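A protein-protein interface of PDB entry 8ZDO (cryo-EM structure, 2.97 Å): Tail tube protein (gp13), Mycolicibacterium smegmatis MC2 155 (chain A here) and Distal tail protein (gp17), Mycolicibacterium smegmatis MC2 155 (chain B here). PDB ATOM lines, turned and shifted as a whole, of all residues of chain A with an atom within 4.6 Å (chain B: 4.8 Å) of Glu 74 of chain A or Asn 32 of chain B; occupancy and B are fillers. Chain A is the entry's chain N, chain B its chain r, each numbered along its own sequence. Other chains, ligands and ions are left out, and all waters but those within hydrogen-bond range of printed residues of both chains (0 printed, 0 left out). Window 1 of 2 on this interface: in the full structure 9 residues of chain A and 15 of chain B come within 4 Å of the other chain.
The backbone carbonyl oxygen (O) of Leu 31 of chain B is in hydrogen-bond range of the backbone NH (N) of Tyr 76 of chain A (2.9 Å).
The backbone carbonyl oxygen of Thr 30 of chain B sits at hydrogen-bond distance from the backbone NH of Gln 71 of chain B. The backbone carbonyl oxygen (O) of Ile 73 of chain A lies within hydrogen-bond range of the backbone NH (N) of Ile 82 of chain A (2.9 Å). O of Ser 69 of chain B sits at hydrogen-bond distance from N of Asn 32 of chain B. ND2 of Asn 32 of chain B sits at hydrogen-bond distance from OE1 of Gln 71 of chain B (3.4 Å).
Ile 73 of chain A touches Gln 71 of chain B (CD1 to NE2, 3.4 Å). O of Glu 74 of chain A touches OD1 of Asn 32 of chain B (3.8 Å). CG of Pro 33 of chain B touches OE1 of Glu 74 of chain A (3.1 Å). Ala 75 of chain A touches Leu 31 of chain B (CA to O, 3.7 Å). CG of Pro 33 of chain B touches O of Ala 75 of chain A, at 3.7 Å. Asn 32 of chain B touches Tyr 76 of chain A. Pro 33 of chain B touches Tyr 76 of chain A (CA to CD1, 3.9 Å).
Glu 74 of chain A touches just these residues of chain B: Asn 32 (3.8 Å) and Pro 33 (3.1 Å). Of the printed residues of chain B, Ala 75 of chain A touches Leu 31 (3.7 Å) and Pro 33 (3.7 Å). Of the printed residues of chain B, Tyr 76 of chain A touches Leu 31, Asn 32 and Pro 33. Of the printed residues of chain A, Leu 31 of chain B touches Ala 75 (3.7 Å) and Tyr 76 (2.9 Å). Of chain A, only Glu 74 and Tyr 76 come within 4 Å of Asn 32 of chain B. Of the printed residues of chain A, Pro 33 of chain B touches Glu 74 (3.1 Å), Ala 75 (3.7 Å) and Tyr 76 (3.9 Å). Asn 34 of chain B touches none of the printed residues of chain A. Of the printed residues of chain A, Gln 71 of chain B touches Ile 73. The nearest printed residue of chain B that does not touch Glu 74 of chain A is Leu 31 of chain B (4.9 Å). The nearest printed residue of chain B that does not touch Ile 73 of chain A is Asn 32 of chain B (5.0 Å).
Printed residues of chain A that touch a printed residue of chain B: Ile 73, Glu 74, Ala 75 and Tyr 76. Hydrophobic or aromatic side chains of chain B within 4 Å of the printed part of chain A: Leu 31 and Pro 33. Among the printed residues, no Asp or Glu carboxylate lies within 4 Å of a Lys or Arg side-chain nitrogen of the other chain.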
ATOM      1  N   ASP A  72      14.802 -15.350 -14.313  1.00  0.00           N
ATOM      2  CA  ASP A  72      15.980 -16.207 -14.329  1.00  0.00           C
ATOM      3  C   ASP A  72      16.522 -16.336 -15.745  1.00  0.00           C
ATOM      4  O   ASP A  72      15.784 -16.682 -16.672  1.00  0.00           O
ATOM      5  CB  ASP A  72      15.644 -17.589 -13.772  1.00  0.00           C
ATOM      6  CG  ASP A  72      15.927 -17.704 -12.288  1.00  0.00           C
ATOM      7  OD1 ASP A  72      16.762 -16.931 -11.777  1.00  0.00           O
ATOM      8  OD2 ASP A  72      15.315 -18.573 -11.633  1.00  0.00           O
ATOM      9  N   ILE A  73      17.810 -16.057 -15.911  1.00  0.00           N
ATOM     10  CA  ILE A  73      18.513 -16.271 -17.165  1.00  0.00           C
ATOM     11  C   ILE A  73      19.282 -17.575 -17.038  1.00  0.00           C
ATOM     12  O   ILE A  73      20.187 -17.695 -16.202  1.00  0.00           O
ATOM     13  CB  ILE A  73      19.457 -15.105 -17.491  1.00  0.00           C
ATOM     14  CG1 ILE A  73      18.697 -13.780 -17.457  1.00  0.00           C
ATOM     15  CG2 ILE A  73      20.115 -15.320 -18.843  1.00  0.00           C
ATOM     16  CD1 ILE A  73      17.745 -13.594 -18.613  1.00  0.00           C
ATOM     17  N   GLU A  74      18.918 -18.549 -17.864  1.00  0.00           N
ATOM     18  CA  GLU A  74      19.484 -19.886 -17.818  1.00  0.00           C
ATOM     19  C   GLU A  74      20.065 -20.243 -19.179  1.00  0.00           C
ATOM     20  O   GLU A  74      19.488 -19.909 -20.219  1.00  0.00           O
ATOM     21  CB  GLU A  74      18.423 -20.901 -17.371  1.00  0.00           C
ATOM     22  CG  GLU A  74      17.157 -20.912 -18.205  1.00  0.00           C
ATOM     23  CD  GLU A  74      17.256 -21.819 -19.404  1.00  0.00           C
ATOM     24  OE1 GLU A  74      18.138 -22.700 -19.401  1.00  0.00           O
ATOM     25  OE2 GLU A  74      16.450 -21.654 -20.344  1.00  0.00           O
ATOM     26  N   ALA A  75      21.214 -20.907 -19.162  1.00  0.00           N
ATOM     27  CA  ALA A  75      22.016 -21.127 -20.355  1.00  0.00           C
ATOM     28  C   ALA A  75      21.783 -22.515 -20.937  1.00  0.00           C
ATOM     29  O   ALA A  75      21.229 -23.408 -20.294  1.00  0.00           O
ATOM     30  CB  ALA A  75      23.503 -20.941 -20.045  1.00  0.00           C
ATOM     31  N   TYR A  76      22.226 -22.678 -22.185  1.00  0.00           N
ATOM     32  CA  TYR A  76      22.071 -23.949 -22.880  1.00  0.00           C
ATOM     33  C   TYR A  76      23.003 -25.013 -22.315  1.00  0.00           C
ATOM     34  O   TYR A  76      22.617 -26.179 -22.189  1.00  0.00           O
ATOM     35  CB  TYR A  76      22.322 -23.746 -24.373  1.00  0.00           C
ATOM     36  CG  TYR A  76      22.466 -25.017 -25.168  1.00  0.00           C
ATOM     37  CD1 TYR A  76      21.360 -25.789 -25.478  1.00  0.00           C
ATOM     38  CD2 TYR A  76      23.704 -25.432 -25.629  1.00  0.00           C
ATOM     39  CE1 TYR A  76      21.484 -26.948 -26.211  1.00  0.00           C
ATOM     40  CE2 TYR A  76      23.838 -26.588 -26.367  1.00  0.00           C
ATOM     41  CZ  TYR A  76      22.724 -27.342 -26.657  1.00  0.00           C
ATOM     42  OH  TYR A  76      22.848 -28.498 -27.389  1.00  0.00           O
ATOM     43  N   GLU A  80      21.445 -25.185 -14.166  1.00  0.00           N
ATOM     44  CA  GLU A  80      20.886 -24.141 -13.324  1.00  0.00           C
ATOM     45  C   GLU A  80      20.934 -22.798 -14.037  1.00  0.00           C
ATOM     46  O   GLU A  80      21.709 -22.609 -14.978  1.00  0.00           O
ATOM     47  CB  GLU A  80      21.657 -24.067 -12.009  1.00  0.00           C
ATOM     48  CG  GLU A  80      23.074 -23.546 -12.163  1.00  0.00           C
ATOM     49  CD  GLU A  80      24.089 -24.661 -12.298  1.00  0.00           C
ATOM     50  OE1 GLU A  80      23.702 -25.840 -12.162  1.00  0.00           O
ATOM     51  OE2 GLU A  80      25.275 -24.362 -12.550  1.00  0.00           O
ATOM     52  N   PRO A  81      20.100 -21.844 -13.625  1.00  0.00           N
ATOM     53  CA  PRO A  81      20.173 -20.502 -14.218  1.00  0.00           C
ATOM     54  C   PRO A  81      21.510 -19.844 -13.919  1.00  0.00           C
ATOM     55  O   PRO A  81      21.948 -19.782 -12.769  1.00  0.00           O
ATOM     56  CB  PRO A  81      19.013 -19.757 -13.550  1.00  0.00           C
ATOM     57  CG  PRO A  81      18.083 -20.828 -13.103  1.00  0.00           C
ATOM     58  CD  PRO A  81      18.957 -21.974 -12.707  1.00  0.00           C
ATOM     59  N   ILE A  82      22.163 -19.349 -14.972  1.00  0.00           N
ATOM     60  CA  ILE A  82      23.456 -18.701 -14.793  1.00  0.00           C
ATOM     61  C   ILE A  82      23.295 -17.376 -14.062  1.00  0.00           C
ATOM     62  O   ILE A  82      24.140 -17.000 -13.241  1.00  0.00           O
ATOM     63  CB  ILE A  82      24.168 -18.520 -16.146  1.00  0.00           C
ATOM     64  CG1 ILE A  82      23.220 -17.935 -17.190  1.00  0.00           C
ATOM     65  CG2 ILE A  82      24.730 -19.843 -16.629  1.00  0.00           C
ATOM     66  CD1 ILE A  82      23.917 -17.502 -18.460  1.00  0.00           C
ATOM     67  N   THR B  30      25.994 -15.505 -24.591  1.00  0.00           N
ATOM     68  CA  THR B  30      25.804 -16.918 -24.297  1.00  0.00           C
ATOM     69  C   THR B  30      24.662 -17.461 -25.144  1.00  0.00           C
ATOM     70  O   THR B  30      23.900 -16.709 -25.751  1.00  0.00           O
ATOM     71  CB  THR B  30      25.513 -17.149 -22.809  1.00  0.00           C
ATOM     72  OG1 THR B  30      24.134 -16.871 -22.541  1.00  0.00           O
ATOM     73  CG2 THR B  30      26.379 -16.251 -21.949  1.00  0.00           C
ATOM     74  N   LEU B  31      24.540 -18.782 -25.183  1.00  0.00           N
ATOM     75  CA  LEU B  31      23.505 -19.449 -25.962  1.00  0.00           C
ATOM     76  C   LEU B  31      22.376 -19.895 -25.044  1.00  0.00           C
ATOM     77  O   LEU B  31      22.629 -20.456 -23.974  1.00  0.00           O
ATOM     78  CB  LEU B  31      24.079 -20.651 -26.713  1.00  0.00           C
ATOM     79  CG  LEU B  31      23.103 -21.450 -27.576  1.00  0.00           C
ATOM     80  CD1 LEU B  31      22.619 -20.614 -28.736  1.00  0.00           C
ATOM     81  CD2 LEU B  31      23.752 -22.723 -28.073  1.00  0.00           C
ATOM     82  N   ASN B  32      21.115 -19.631 -25.462  1.00  0.00           N
ATOM     83  CA  ASN B  32      19.913 -20.029 -24.754  1.00  0.00           C
ATOM     84  C   ASN B  32      19.444 -21.395 -25.238  1.00  0.00           C
ATOM     85  O   ASN B  32      19.744 -21.798 -26.366  1.00  0.00           O
ATOM     86  CB  ASN B  32      18.807 -19.003 -24.975  1.00  0.00           C
ATOM     87  CG  ASN B  32      19.084 -17.691 -24.279  1.00  0.00           C
ATOM     88  OD1 ASN B  32      19.769 -17.649 -23.260  1.00  0.00           O
ATOM     89  ND2 ASN B  32      18.555 -16.608 -24.830  1.00  0.00           N
ATOM     90  N   PRO B  33      18.708 -22.135 -24.410  1.00  0.00           N
ATOM     91  CA  PRO B  33      18.249 -23.466 -24.826  1.00  0.00           C
ATOM     92  C   PRO B  33      17.219 -23.427 -25.941  1.00  0.00           C
ATOM     93  O   PRO B  33      16.852 -22.353 -26.429  1.00  0.00           O
ATOM     94  CB  PRO B  33      17.647 -24.046 -23.539  1.00  0.00           C
ATOM     95  CG  PRO B  33      18.219 -23.232 -22.447  1.00  0.00           C
ATOM     96  CD  PRO B  33      18.397 -21.867 -22.999  1.00  0.00           C
ATOM     97  N   ASN B  34      16.753 -24.607 -26.351  1.00  0.00           N
ATOM     98  CA  ASN B  34      15.710 -24.760 -27.364  1.00  0.00           C
ATOM     99  C   ASN B  34      16.153 -24.194 -28.715  1.00  0.00           C
ATOM    100  O   ASN B  34      15.583 -23.236 -29.240  1.00  0.00           O
ATOM    101  CB  ASN B  34      14.396 -24.124 -26.901  1.00  0.00           C
ATOM    102  CG  ASN B  34      13.211 -24.573 -27.728  1.00  0.00           C
ATOM    103  OD1 ASN B  34      13.255 -25.618 -28.378  1.00  0.00           O
ATOM    104  ND2 ASN B  34      12.143 -23.785 -27.711  1.00  0.00           N
ATOM    105  N   SER B  69      18.317 -18.741 -29.811  1.00  0.00           N
ATOM    106  CA  SER B  69      18.381 -17.493 -29.072  1.00  0.00           C
ATOM    107  C   SER B  69      19.739 -17.357 -28.403  1.00  0.00           C
ATOM    108  O   SER B  69      20.317 -18.341 -27.932  1.00  0.00           O
ATOM    109  CB  SER B  69      17.269 -17.419 -28.025  1.00  0.00           C
ATOM    110  OG  SER B  69      17.212 -16.136 -27.431  1.00  0.00           O
ATOM    111  N   VAL B  70      20.249 -16.134 -28.371  1.00  0.00           N
ATOM    112  CA  VAL B  70      21.457 -15.829 -27.622  1.00  0.00           C
ATOM    113  C   VAL B  70      21.110 -14.747 -26.616  1.00  0.00           C
ATOM    114  O   VAL B  70      20.102 -14.056 -26.736  1.00  0.00           O
ATOM    115  CB  VAL B  70      22.622 -15.387 -28.527  1.00  0.00           C
ATOM    116  CG1 VAL B  70      23.114 -16.556 -29.355  1.00  0.00           C
ATOM    117  CG2 VAL B  70      22.192 -14.245 -29.419  1.00  0.00           C
ATOM    118  N   GLN B  71      21.947 -14.624 -25.598  1.00  0.00           N
ATOM    119  CA  GLN B  71      21.773 -13.619 -24.562  1.00  0.00           C
ATOM    120  C   GLN B  71      23.033 -12.776 -24.497  1.00  0.00           C
ATOM    121  O   GLN B  71      24.114 -13.298 -24.205  1.00  0.00           O
ATOM    122  CB  GLN B  71      21.482 -14.265 -23.208  1.00  0.00           C
ATOM    123  CG  GLN B  71      20.988 -13.298 -22.156  1.00  0.00           C
ATOM    124  CD  GLN B  71      19.481 -13.217 -22.106  1.00  0.00           C
ATOM    125  OE1 GLN B  71      18.784 -14.060 -22.666  1.00  0.00           O
ATOM    126  NE2 GLN B  71      18.968 -12.198 -21.433  1.00  0.00           N
ATOM    127  N   PRO B 133      17.938 -10.800 -24.819  1.00  0.00           N
ATOM    128  CA  PRO B 133      18.030 -11.916 -25.762  1.00  0.00           C
ATOM    129  C   PRO B 133      17.802 -11.491 -27.203  1.00  0.00           C
ATOM    130  O   PRO B 133      16.941 -10.669 -27.516  1.00  0.00           O
ATOM    131  CB  PRO B 133      16.902 -12.841 -25.289  1.00  0.00           C
ATOM    132  CG  PRO B 133      15.868 -11.899 -24.758  1.00  0.00           C
ATOM    133  CD  PRO B 133      16.568 -10.634 -24.310  1.00  0.00           C
